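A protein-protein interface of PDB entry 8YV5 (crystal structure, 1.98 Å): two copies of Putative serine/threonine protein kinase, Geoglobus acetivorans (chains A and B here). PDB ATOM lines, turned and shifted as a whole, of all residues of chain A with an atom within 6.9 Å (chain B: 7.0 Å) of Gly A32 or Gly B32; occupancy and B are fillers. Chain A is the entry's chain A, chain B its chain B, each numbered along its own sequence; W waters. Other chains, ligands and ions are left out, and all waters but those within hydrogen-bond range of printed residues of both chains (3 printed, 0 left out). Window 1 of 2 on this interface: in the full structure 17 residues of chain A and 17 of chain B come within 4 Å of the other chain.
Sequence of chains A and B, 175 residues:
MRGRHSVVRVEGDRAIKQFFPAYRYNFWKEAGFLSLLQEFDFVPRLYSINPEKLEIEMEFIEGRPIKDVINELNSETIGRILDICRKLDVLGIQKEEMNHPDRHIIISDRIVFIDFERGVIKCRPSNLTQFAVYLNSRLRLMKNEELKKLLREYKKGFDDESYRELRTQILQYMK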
ATOM      1  N   ASN A  26      19.697 -24.211  -5.184  1.00  0.00           N
ATOM      2  CA  ASN A  26      18.550 -24.779  -4.479  1.00  0.00           C
ATOM      3  C   ASN A  26      18.943 -25.661  -3.317  1.00  0.00           C
ATOM      4  O   ASN A  26      18.194 -25.755  -2.329  1.00  0.00           O
ATOM      5  CB  ASN A  26      17.712 -25.573  -5.465  1.00  0.00           C
ATOM      6  CG  ASN A  26      17.262 -24.725  -6.620  1.00  0.00           C
ATOM      7  OD1 ASN A  26      17.930 -24.681  -7.654  1.00  0.00           O
ATOM      8  ND2 ASN A  26      16.148 -24.026  -6.455  1.00  0.00           N
ATOM      9  N   PHE A  27      20.068 -26.361  -3.444  1.00  0.00           N
ATOM     10  CA  PHE A  27      20.624 -27.116  -2.330  1.00  0.00           C
ATOM     11  C   PHE A  27      20.685 -26.263  -1.077  1.00  0.00           C
ATOM     12  O   PHE A  27      20.266 -26.691   0.004  1.00  0.00           O
ATOM     13  CB  PHE A  27      22.033 -27.636  -2.711  1.00  0.00           C
ATOM     14  CG  PHE A  27      22.848 -28.104  -1.533  1.00  0.00           C
ATOM     15  CD1 PHE A  27      22.626 -29.359  -0.988  1.00  0.00           C
ATOM     16  CD2 PHE A  27      23.856 -27.300  -0.974  1.00  0.00           C
ATOM     17  CE1 PHE A  27      23.360 -29.812   0.109  1.00  0.00           C
ATOM     18  CE2 PHE A  27      24.602 -27.749   0.137  1.00  0.00           C
ATOM     19  CZ  PHE A  27      24.354 -29.005   0.672  1.00  0.00           C
ATOM     20  N   TRP A  28      21.255 -25.055  -1.197  1.00  0.00           N
ATOM     21  CA  TRP A  28      21.450 -24.216  -0.009  1.00  0.00           C
ATOM     22  C   TRP A  28      20.137 -23.668   0.526  1.00  0.00           C
ATOM     23  O   TRP A  28      20.031 -23.419   1.728  1.00  0.00           O
ATOM     24  CB  TRP A  28      22.397 -23.043  -0.333  1.00  0.00           C
ATOM     25  CG  TRP A  28      23.854 -23.508  -0.422  1.00  0.00           C
ATOM     26  CD1 TRP A  28      24.680 -23.477  -1.525  1.00  0.00           C
ATOM     27  CD2 TRP A  28      24.620 -24.084   0.640  1.00  0.00           C
ATOM     28  NE1 TRP A  28      25.930 -23.981  -1.187  1.00  0.00           N
ATOM     29  CE2 TRP A  28      25.915 -24.363   0.131  1.00  0.00           C
ATOM     30  CE3 TRP A  28      24.344 -24.383   1.979  1.00  0.00           C
ATOM     31  CZ2 TRP A  28      26.928 -24.947   0.915  1.00  0.00           C
ATOM     32  CZ3 TRP A  28      25.368 -24.936   2.777  1.00  0.00           C
ATOM     33  CH2 TRP A  28      26.651 -25.205   2.232  1.00  0.00           C
ATOM     34  N   LYS A  29      19.138 -23.419  -0.342  1.00  0.00           N
ATOM     35  CA  LYS A  29      17.878 -22.937   0.209  1.00  0.00           C
ATOM     36  C   LYS A  29      17.147 -24.046   0.929  1.00  0.00           C
ATOM     37  O   LYS A  29      16.581 -23.823   2.013  1.00  0.00           O
ATOM     38  CB  LYS A  29      16.992 -22.342  -0.880  1.00  0.00           C
ATOM     39  CG  LYS A  29      17.783 -21.307  -1.680  1.00  0.00           C
ATOM     40  CD  LYS A  29      18.381 -20.148  -0.802  1.00  0.00           C
ATOM     41  CE  LYS A  29      19.177 -19.143  -1.700  1.00  0.00           C
ATOM     42  NZ  LYS A  29      19.847 -17.992  -0.999  1.00  0.00           N
ATOM     43  N   GLU A  30      17.155 -25.254   0.357  1.00  0.00           N
ATOM     44  CA  GLU A  30      16.620 -26.408   1.079  1.00  0.00           C
ATOM     45  C   GLU A  30      17.287 -26.554   2.443  1.00  0.00           C
ATOM     46  O   GLU A  30      16.618 -26.623   3.474  1.00  0.00           O
ATOM     47  CB  GLU A  30      16.844 -27.683   0.266  1.00  0.00           C
ATOM     48  CG  GLU A  30      16.227 -28.961   0.851  1.00  0.00           C
ATOM     49  CD  GLU A  30      14.712 -29.046   0.546  1.00  0.00           C
ATOM     50  OE1 GLU A  30      14.351 -29.280  -0.628  1.00  0.00           O
ATOM     51  OE2 GLU A  30      13.874 -28.951   1.473  1.00  0.00           O
ATOM     52  N   ALA A  31      18.612 -26.589   2.471  1.00  0.00           N
ATOM     53  CA  ALA A  31      19.300 -26.691   3.761  1.00  0.00           C
ATOM     54  C   ALA A  31      18.929 -25.540   4.686  1.00  0.00           C
ATOM     55  O   ALA A  31      18.704 -25.754   5.890  1.00  0.00           O
ATOM     56  CB  ALA A  31      20.819 -26.710   3.547  1.00  0.00           C
ATOM     57  N   GLY A  32      18.904 -24.307   4.150  1.00  0.00           N
ATOM     58  CA  GLY A  32      18.669 -23.136   4.991  1.00  0.00           C
ATOM     59  C   GLY A  32      17.289 -23.133   5.625  1.00  0.00           C
ATOM     60  O   GLY A  32      17.153 -22.992   6.839  1.00  0.00           O
ATOM     61  N   PHE A  33      16.248 -23.321   4.815  1.00  0.00           N
ATOM     62  CA  PHE A  33      14.900 -23.256   5.360  1.00  0.00           C
ATOM     63  C   PHE A  33      14.589 -24.465   6.248  1.00  0.00           C
ATOM     64  O   PHE A  33      13.938 -24.307   7.284  1.00  0.00           O
ATOM     65  CB  PHE A  33      13.879 -23.089   4.211  1.00  0.00           C
ATOM     66  CG  PHE A  33      13.956 -21.703   3.537  1.00  0.00           C
ATOM     67  CD1 PHE A  33      13.725 -20.534   4.272  1.00  0.00           C
ATOM     68  CD2 PHE A  33      14.331 -21.576   2.202  1.00  0.00           C
ATOM     69  CE1 PHE A  33      13.833 -19.250   3.656  1.00  0.00           C
ATOM     70  CE2 PHE A  33      14.452 -20.308   1.570  1.00  0.00           C
ATOM     71  CZ  PHE A  33      14.195 -19.142   2.301  1.00  0.00           C
ATOM     72  N   LEU A  34      15.091 -25.661   5.923  1.00  0.00           N
ATOM     73  CA  LEU A  34      14.928 -26.768   6.870  1.00  0.00           C
ATOM     74  C   LEU A  34      15.570 -26.427   8.220  1.00  0.00           C
ATOM     75  O   LEU A  34      14.973 -26.634   9.283  1.00  0.00           O
ATOM     76  CB  LEU A  34      15.552 -28.040   6.277  1.00  0.00           C
ATOM     77  CG  LEU A  34      14.717 -28.733   5.219  1.00  0.00           C
ATOM     78  CD1 LEU A  34      15.511 -29.929   4.712  1.00  0.00           C
ATOM     79  CD2 LEU A  34      13.410 -29.222   5.902  1.00  0.00           C
ATOM     80  N   SER A  35      16.781 -25.863   8.196  1.00  0.00           N
ATOM     81  CA  SER A  35      17.439 -25.478   9.452  1.00  0.00           C
ATOM     82  C   SER A  35      16.603 -24.469  10.226  1.00  0.00           C
ATOM     83  O   SER A  35      16.344 -24.645  11.424  1.00  0.00           O
ATOM     84  CB  SER A  35      18.835 -24.899   9.158  1.00  0.00           C
ATOM     85  OG  SER A  35      19.705 -25.928   8.710  1.00  0.00           O
ATOM     86  N   LEU A  36      16.117 -23.424   9.541  1.00  0.00           N
ATOM     87  CA  LEU A  36      15.358 -22.383  10.235  1.00  0.00           C
ATOM     88  C   LEU A  36      14.023 -22.898  10.748  1.00  0.00           C
ATOM     89  O   LEU A  36      13.432 -22.261  11.623  1.00  0.00           O
ATOM     90  CB  LEU A  36      15.093 -21.190   9.310  1.00  0.00           C
ATOM     91  CG  LEU A  36      16.366 -20.410   8.942  1.00  0.00           C
ATOM     92  CD1 LEU A  36      15.981 -19.222   8.111  1.00  0.00           C
ATOM     93  CD2 LEU A  36      17.115 -19.998  10.179  1.00  0.00           C
ATOM     94  N   LEU A  37      13.556 -24.053  10.261  1.00  0.00           N
ATOM     95  CA  LEU A  37      12.259 -24.562  10.687  1.00  0.00           C
ATOM     96  C   LEU A  37      12.348 -25.717  11.673  1.00  0.00           C
ATOM     97  O   LEU A  37      11.307 -26.233  12.077  1.00  0.00           O
ATOM     98  CB  LEU A  37      11.419 -24.969   9.461  1.00  0.00           C
ATOM     99  CG  LEU A  37      11.051 -23.708   8.648  1.00  0.00           C
ATOM    100  CD1 LEU A  37      10.451 -24.008   7.298  1.00  0.00           C
ATOM    101  CD2 LEU A  37      10.095 -22.806   9.426  1.00  0.00           C
ATOM    102  N   LEU A  46      16.510 -32.445  10.319  1.00  0.00           N
ATOM    103  CA  LEU A  46      17.665 -32.340   9.425  1.00  0.00           C
ATOM    104  C   LEU A  46      18.882 -32.988  10.080  1.00  0.00           C
ATOM    105  O   LEU A  46      19.171 -32.727  11.248  1.00  0.00           O
ATOM    106  CB  LEU A  46      17.923 -30.859   9.109  1.00  0.00           C
ATOM    107  CG  LEU A  46      19.120 -30.524   8.234  1.00  0.00           C
ATOM    108  CD1 LEU A  46      19.053 -31.293   6.998  1.00  0.00           C
ATOM    109  CD2 LEU A  46      19.059 -29.053   7.894  1.00  0.00           C
ATOM    110  N   ILE A  49      24.408 -32.085   6.087  1.00  0.00           N
ATOM    111  CA  ILE A  49      24.517 -31.485   4.767  1.00  0.00           C
ATOM    112  C   ILE A  49      25.898 -31.847   4.248  1.00  0.00           C
ATOM    113  O   ILE A  49      26.850 -32.019   5.017  1.00  0.00           O
ATOM    114  CB  ILE A  49      24.318 -29.963   4.779  1.00  0.00           C
ATOM    115  CG1 ILE A  49      25.397 -29.313   5.622  1.00  0.00           C
ATOM    116  CG2 ILE A  49      22.936 -29.574   5.336  1.00  0.00           C
ATOM    117  CD1 ILE A  49      25.629 -27.853   5.233  1.00  0.00           C
ATOM    118  N   ILE A  56      21.552 -33.609   1.142  1.00  0.00           N
ATOM    119  CA  ILE A  56      20.932 -33.320   2.429  1.00  0.00           C
ATOM    120  C   ILE A  56      20.355 -34.613   2.962  1.00  0.00           C
ATOM    121  O   ILE A  56      19.598 -35.274   2.245  1.00  0.00           O
ATOM    122  CB  ILE A  56      19.825 -32.272   2.282  1.00  0.00           C
ATOM    123  CG1 ILE A  56      20.476 -30.957   1.809  1.00  0.00           C
ATOM    124  CG2 ILE A  56      19.139 -32.083   3.597  1.00  0.00           C
ATOM    125  CD1 ILE A  56      19.502 -29.851   1.615  1.00  0.00           C
ATOM    126  N   PHE A 116      11.700 -27.464   0.403  1.00  0.00           N
ATOM    127  CA  PHE A 116      11.882 -26.030   0.595  1.00  0.00           C
ATOM    128  C   PHE A 116      12.897 -25.442  -0.366  1.00  0.00           C
ATOM    129  O   PHE A 116      13.283 -24.278  -0.204  1.00  0.00           O
ATOM    130  CB  PHE A 116      12.280 -25.751   2.043  1.00  0.00           C
ATOM    131  CG  PHE A 116      11.137 -25.981   2.996  1.00  0.00           C
ATOM    132  CD1 PHE A 116      10.872 -27.261   3.492  1.00  0.00           C
ATOM    133  CD2 PHE A 116      10.276 -24.956   3.298  1.00  0.00           C
ATOM    134  CE1 PHE A 116       9.782 -27.482   4.344  1.00  0.00           C
ATOM    135  CE2 PHE A 116       9.188 -25.156   4.137  1.00  0.00           C
ATOM    136  CZ  PHE A 116       8.932 -26.430   4.662  1.00  0.00           C
ATOM    137  N   ASN B  26      19.798 -21.734  18.867  1.00  0.00           N
ATOM    138  CA  ASN B  26      20.695 -20.854  18.140  1.00  0.00           C
ATOM    139  C   ASN B  26      21.577 -21.605  17.166  1.00  0.00           C
ATOM    140  O   ASN B  26      21.986 -21.047  16.127  1.00  0.00           O
ATOM    141  CB  ASN B  26      21.541 -20.112  19.156  1.00  0.00           C
ATOM    142  CG  ASN B  26      20.672 -19.328  20.128  1.00  0.00           C
ATOM    143  OD1 ASN B  26      20.469 -19.751  21.249  1.00  0.00           O
ATOM    144  ND2 ASN B  26      20.158 -18.173  19.684  1.00  0.00           N
ATOM    145  N   PHE B  27      21.932 -22.839  17.515  1.00  0.00           N
ATOM    146  CA  PHE B  27      22.632 -23.685  16.556  1.00  0.00           C
ATOM    147  C   PHE B  27      21.909 -23.679  15.214  1.00  0.00           C
ATOM    148  O   PHE B  27      22.522 -23.506  14.160  1.00  0.00           O
ATOM    149  CB  PHE B  27      22.736 -25.109  17.135  1.00  0.00           C
ATOM    150  CG  PHE B  27      23.079 -26.155  16.116  1.00  0.00           C
ATOM    151  CD1 PHE B  27      24.389 -26.356  15.742  1.00  0.00           C
ATOM    152  CD2 PHE B  27      22.088 -26.998  15.582  1.00  0.00           C
ATOM    153  CE1 PHE B  27      24.753 -27.341  14.802  1.00  0.00           C
ATOM    154  CE2 PHE B  27      22.433 -28.014  14.665  1.00  0.00           C
ATOM    155  CZ  PHE B  27      23.767 -28.171  14.245  1.00  0.00           C
ATOM    156  N   TRP B  28      20.592 -23.908  15.233  1.00  0.00           N
ATOM    157  CA  TRP B  28      19.837 -24.004  13.983  1.00  0.00           C
ATOM    158  C   TRP B  28      19.741 -22.673  13.254  1.00  0.00           C
ATOM    159  O   TRP B  28      19.668 -22.649  12.027  1.00  0.00           O
ATOM    160  CB  TRP B  28      18.417 -24.502  14.280  1.00  0.00           C
ATOM    161  CG  TRP B  28      18.408 -26.015  14.555  1.00  0.00           C
ATOM    162  CD1 TRP B  28      18.012 -26.649  15.702  1.00  0.00           C
ATOM    163  CD2 TRP B  28      18.884 -27.038  13.669  1.00  0.00           C
ATOM    164  NE1 TRP B  28      18.168 -28.020  15.561  1.00  0.00           N
ATOM    165  CE2 TRP B  28      18.699 -28.278  14.321  1.00  0.00           C
ATOM    166  CE3 TRP B  28      19.417 -27.025  12.362  1.00  0.00           C
ATOM    167  CZ2 TRP B  28      19.030 -29.489  13.725  1.00  0.00           C
ATOM    168  CZ3 TRP B  28      19.756 -28.210  11.785  1.00  0.00           C
ATOM    169  CH2 TRP B  28      19.556 -29.441  12.461  1.00  0.00           C
ATOM    170  N   LYS B  29      19.702 -21.563  13.972  1.00  0.00           N
ATOM    171  CA  LYS B  29      19.664 -20.283  13.254  1.00  0.00           C
ATOM    172  C   LYS B  29      21.016 -19.976  12.617  1.00  0.00           C
ATOM    173  O   LYS B  29      21.085 -19.456  11.482  1.00  0.00           O
ATOM    174  CB  LYS B  29      19.226 -19.155  14.199  1.00  0.00           C
ATOM    175  CG  LYS B  29      17.817 -19.336  14.788  1.00  0.00           C
ATOM    176  CD  LYS B  29      16.733 -19.879  13.803  1.00  0.00           C
ATOM    177  CE  LYS B  29      15.408 -20.139  14.556  1.00  0.00           C
ATOM    178  NZ  LYS B  29      14.208 -20.733  13.814  1.00  0.00           N
ATOM    179  N   GLU B  30      22.112 -20.292  13.317  1.00  0.00           N
ATOM    180  CA  GLU B  30      23.428 -20.170  12.691  1.00  0.00           C
ATOM    181  C   GLU B  30      23.512 -21.001  11.409  1.00  0.00           C
ATOM    182  O   GLU B  30      23.853 -20.481  10.338  1.00  0.00           O
ATOM    183  CB  GLU B  30      24.520 -20.580  13.683  1.00  0.00           C
ATOM    184  CG  GLU B  30      25.949 -20.381  13.144  1.00  0.00           C
ATOM    185  CD  GLU B  30      26.433 -18.960  13.406  1.00  0.00           C
ATOM    186  OE1 GLU B  30      26.517 -18.556  14.587  1.00  0.00           O
ATOM    187  OE2 GLU B  30      26.672 -18.239  12.401  1.00  0.00           O
ATOM    188  N   ALA B  31      23.175 -22.289  11.505  1.00  0.00           N
ATOM    189  CA  ALA B  31      23.162 -23.175  10.337  1.00  0.00           C
ATOM    190  C   ALA B  31      22.266 -22.641   9.233  1.00  0.00           C
ATOM    191  O   ALA B  31      22.657 -22.626   8.053  1.00  0.00           O
ATOM    192  CB  ALA B  31      22.666 -24.559  10.742  1.00  0.00           C
ATOM    193  N   GLY B  32      21.052 -22.210   9.595  1.00  0.00           N
ATOM    194  CA  GLY B  32      20.095 -21.776   8.584  1.00  0.00           C
ATOM    195  C   GLY B  32      20.549 -20.530   7.832  1.00  0.00           C
ATOM    196  O   GLY B  32      20.497 -20.475   6.596  1.00  0.00           O
ATOM    197  N   PHE B  33      20.952 -19.490   8.564  1.00  0.00           N
ATOM    198  CA  PHE B  33      21.286 -18.235   7.885  1.00  0.00           C
ATOM    199  C   PHE B  33      22.607 -18.338   7.131  1.00  0.00           C
ATOM    200  O   PHE B  33      22.749 -17.755   6.049  1.00  0.00           O
ATOM    201  CB  PHE B  33      21.296 -17.077   8.891  1.00  0.00           C
ATOM    202  CG  PHE B  33      19.884 -16.675   9.340  1.00  0.00           C
ATOM    203  CD1 PHE B  33      18.950 -16.239   8.405  1.00  0.00           C
ATOM    204  CD2 PHE B  33      19.480 -16.817  10.668  1.00  0.00           C
ATOM    205  CE1 PHE B  33      17.656 -15.924   8.783  1.00  0.00           C
ATOM    206  CE2 PHE B  33      18.171 -16.496  11.064  1.00  0.00           C
ATOM    207  CZ  PHE B  33      17.260 -16.055  10.114  1.00  0.00           C
ATOM    208  N   LEU B  34      23.594 -19.071   7.671  1.00  0.00           N
ATOM    209  CA  LEU B  34      24.798 -19.309   6.869  1.00  0.00           C
ATOM    210  C   LEU B  34      24.435 -20.017   5.566  1.00  0.00           C
ATOM    211  O   LEU B  34      24.962 -19.686   4.501  1.00  0.00           O
ATOM    212  CB  LEU B  34      25.822 -20.138   7.663  1.00  0.00           C
ATOM    213  CG  LEU B  34      26.643 -19.447   8.772  1.00  0.00           C
ATOM    214  CD1 LEU B  34      27.463 -20.479   9.507  1.00  0.00           C
ATOM    215  CD2 LEU B  34      27.584 -18.339   8.178  1.00  0.00           C
ATOM    216  N   SER B  35      23.555 -21.018   5.631  1.00  0.00           N
ATOM    217  CA  SER B  35      23.140 -21.717   4.412  1.00  0.00           C
ATOM    218  C   SER B  35      22.491 -20.763   3.421  1.00  0.00           C
ATOM    219  O   SER B  35      22.790 -20.800   2.214  1.00  0.00           O
ATOM    220  CB  SER B  35      22.152 -22.855   4.752  1.00  0.00           C
ATOM    221  OG  SER B  35      22.821 -23.835   5.542  1.00  0.00           O
ATOM    222  N   LEU B  36      21.572 -19.923   3.905  1.00  0.00           N
ATOM    223  CA  LEU B  36      20.845 -19.034   3.003  1.00  0.00           C
ATOM    224  C   LEU B  36      21.749 -17.966   2.420  1.00  0.00           C
ATOM    225  O   LEU B  36      21.365 -17.310   1.445  1.00  0.00           O
ATOM    226  CB  LEU B  36      19.693 -18.341   3.732  1.00  0.00           C
ATOM    227  CG  LEU B  36      18.549 -19.269   4.161  1.00  0.00           C
ATOM    228  CD1 LEU B  36      17.473 -18.362   4.709  1.00  0.00           C
ATOM    229  CD2 LEU B  36      18.056 -20.099   2.991  1.00  0.00           C
ATOM    230  N   LEU B  37      22.921 -17.771   2.990  1.00  0.00           N
ATOM    231  CA  LEU B  37      23.829 -16.723   2.529  1.00  0.00           C
ATOM    232  C   LEU B  37      25.009 -17.261   1.727  1.00  0.00           C
ATOM    233  O   LEU B  37      25.855 -16.457   1.271  1.00  0.00           O
ATOM    234  CB  LEU B  37      24.328 -15.915   3.746  1.00  0.00           C
ATOM    235  CG  LEU B  37      23.164 -15.089   4.349  1.00  0.00           C
ATOM    236  CD1 LEU B  37      23.566 -14.436   5.664  1.00  0.00           C
ATOM    237  CD2 LEU B  37      22.625 -14.018   3.363  1.00  0.00           C
ATOM    238  N   LEU B  46      30.071 -22.823   4.456  1.00  0.00           N
ATOM    239  CA  LEU B  46      29.578 -23.786   5.430  1.00  0.00           C
ATOM    240  C   LEU B  46      29.936 -25.184   4.933  1.00  0.00           C
ATOM    241  O   LEU B  46      29.699 -25.499   3.765  1.00  0.00           O
ATOM    242  CB  LEU B  46      28.059 -23.628   5.611  1.00  0.00           C
ATOM    243  CG  LEU B  46      27.316 -24.593   6.519  1.00  0.00           C
ATOM    244  CD1 LEU B  46      27.949 -24.618   7.833  1.00  0.00           C
ATOM    245  CD2 LEU B  46      25.858 -24.167   6.682  1.00  0.00           C
ATOM    246  N   ILE B  49      27.206 -29.741   9.305  1.00  0.00           N
ATOM    247  CA  ILE B  49      26.531 -29.569  10.571  1.00  0.00           C
ATOM    248  C   ILE B  49      26.443 -30.934  11.252  1.00  0.00           C
ATOM    249  O   ILE B  49      26.427 -31.982  10.599  1.00  0.00           O
ATOM    250  CB  ILE B  49      25.145 -28.944  10.381  1.00  0.00           C
ATOM    251  CG1 ILE B  49      24.209 -29.987   9.765  1.00  0.00           C
ATOM    252  CG2 ILE B  49      25.241 -27.665   9.554  1.00  0.00           C
ATOM    253  CD1 ILE B  49      22.741 -29.588   9.770  1.00  0.00           C
ATOM    254  N   ILE B  56      28.921 -26.738  14.111  1.00  0.00           N
ATOM    255  CA  ILE B  56      28.960 -26.234  12.740  1.00  0.00           C
ATOM    256  C   ILE B  56      30.415 -26.106  12.317  1.00  0.00           C
ATOM    257  O   ILE B  56      31.215 -25.513  13.050  1.00  0.00           O
ATOM    258  CB  ILE B  56      28.204 -24.902  12.630  1.00  0.00           C
ATOM    259  CG1 ILE B  56      26.708 -25.141  12.919  1.00  0.00           C
ATOM    260  CG2 ILE B  56      28.441 -24.201  11.286  1.00  0.00           C
ATOM    261  CD1 ILE B  56      25.988 -23.878  13.022  1.00  0.00           C
ATOM    262  N   ILE B  93      17.067 -10.403   6.331  1.00  0.00           N
ATOM    263  CA  ILE B  93      17.734 -11.089   7.441  1.00  0.00           C
ATOM    264  C   ILE B  93      18.226 -10.049   8.431  1.00  0.00           C
ATOM    265  O   ILE B  93      19.105  -9.233   8.107  1.00  0.00           O
ATOM    266  CB  ILE B  93      18.862 -12.009   6.954  1.00  0.00           C
ATOM    267  CG1 ILE B  93      18.234 -13.121   6.101  1.00  0.00           C
ATOM    268  CG2 ILE B  93      19.697 -12.572   8.147  1.00  0.00           C
ATOM    269  CD1 ILE B  93      19.199 -13.817   5.141  1.00  0.00           C
ATOM    270  N   PHE B 116      25.727 -15.633  13.085  1.00  0.00           N
ATOM    271  CA  PHE B 116      24.325 -15.376  12.686  1.00  0.00           C
ATOM    272  C   PHE B 116      23.378 -16.147  13.611  1.00  0.00           C
ATOM    273  O   PHE B 116      22.206 -16.281  13.262  1.00  0.00           O
ATOM    274  CB  PHE B 116      24.122 -15.797  11.233  1.00  0.00           C
ATOM    275  CG  PHE B 116      24.731 -14.868  10.214  1.00  0.00           C
ATOM    276  CD1 PHE B 116      26.058 -14.995   9.844  1.00  0.00           C
ATOM    277  CD2 PHE B 116      23.977 -13.866   9.630  1.00  0.00           C
ATOM    278  CE1 PHE B 116      26.618 -14.139   8.910  1.00  0.00           C
ATOM    279  CE2 PHE B 116      24.539 -13.010   8.698  1.00  0.00           C
ATOM    280  CZ  PHE B 116      25.857 -13.148   8.341  1.00  0.00           C
HETATM  281  O   HOH W   1      22.489 -19.561  -0.333  1.00  0.00           O
HETATM  282  O   HOH W   2      26.615 -32.151   7.817  1.00  0.00           O
HETATM  283  O   HOH W   3      14.944 -23.554  13.731  1.00  0.00           O
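Of the 17 printed residues of chain B, 8 touch a printed residue of chain A. Printed residues of chain B that touch a printed residue of chain A: Trp B28, Lys B29, Ala B31, Gly B32, Phe B33, Ser B35, Leu B36 and Leu B46. Hydrophobic or aromatic side chains of chain B that line the printed part of chain A: Trp B28, Ala B31, Phe B33, Leu B36 and Leu B46. Of the 16 printed residues of chain A, 8 touch a printed residue of chain B. Hydrophobic or aromatic side chains of chain A that line the printed part of chain B: Trp A28, Phe A33, Leu A36, Leu A46 and Ile A49.
Water W2 lies within hydrogen-bond range of O of Ile B49 (2.8 Å) and N of Ile A49 (2.8 Å). Water W1 lies within hydrogen-bond range of O of Ser B35, O of Leu B36 and NZ of Lys A29. Water W3 lies within hydrogen-bond range of the backbone carbonyl oxygen (O) of Leu A36, the backbone carbonyl oxygen (O) of Ser A35 and the side-chain amino group (NZ) of Lys B29.
The backbone carbonyl oxygen (O) of Leu A36 is in hydrogen-bond range of the side-chain amino group (NZ) of Lys B29 (2.8 Å). NZ of Lys A29 lies within hydrogen-bond range of O of Leu B36, 3.0 Å away.
Trp A28 touches Leu B46, and with the chains exchanged Leu A46 touches Trp B28. Gly A32 touches Ser B35, and with the chains exchanged Ser A35 touches Gly B32. Phe A33 touches Leu B36, and with the chains exchanged Leu A36 touches Phe B33. Ser A35 touches Ala B31, but with the chains exchanged Ala A31 does not touch Ser B35 (4.03 Å).
CB of Trp A28 touches O of Ser B35, at 3.4 Å. CH2 of Trp A28 touches O of Leu B46 (3.4 Å). CB of Ser B35 touches CA of Gly A32, at 3.5 Å. Gly A32 touches Leu B36 (CA to CD2, 3.7 Å). CB of Ala B31 touches OG of Ser A35, 3.8 Å away. Gly B32 touches Ser A35. Phe B33 touches Leu A36 (CE1 to CD1, 3.8 Å). Leu B36 touches Leu A36. O of Leu A46 touches CH2 of Trp B28 (3.5 Å). Ile A49 touches Leu B46 (CD1 to CG, 3.9 Å).
Gly A32 touches just these residues of chain B: Gly B32, Ser B35 and Leu B36. Of the printed residues of chain B, Ser A35 touches Trp B28, Ala B31 and Gly B32. Leu A37 touches none of the printed residues of chain B. Of the printed residues of chain B, Leu A46 touches Trp B28. Printed residues of chain A within 4 Å of Trp B28: Ser A35 (3.5 Å) and Leu A46 (3.5 Å). Of the printed residues of chain A, Lys B29 touches Leu A36 (2.8 Å). Gly B32 touches just these residues of chain A: Gly A32, Ser A35 and Leu A36. The nearest residue of chain A that does not touch Gly B32 is Ala A31 (5.0 Å). The nearest printed residue of chain A that does not touch Leu B46 is Ala A31 (6.5 Å).
The side-chain hydroxyl of Ser B35 is in hydrogen-bond range of the backbone carbonyl oxygen of Ala B31 (2.8 Å). The side-chain hydroxyl (OG) of Ser A35 is in hydrogen-bond range of the backbone carbonyl oxygen (O) of Ala A31, at 3.0 Å.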
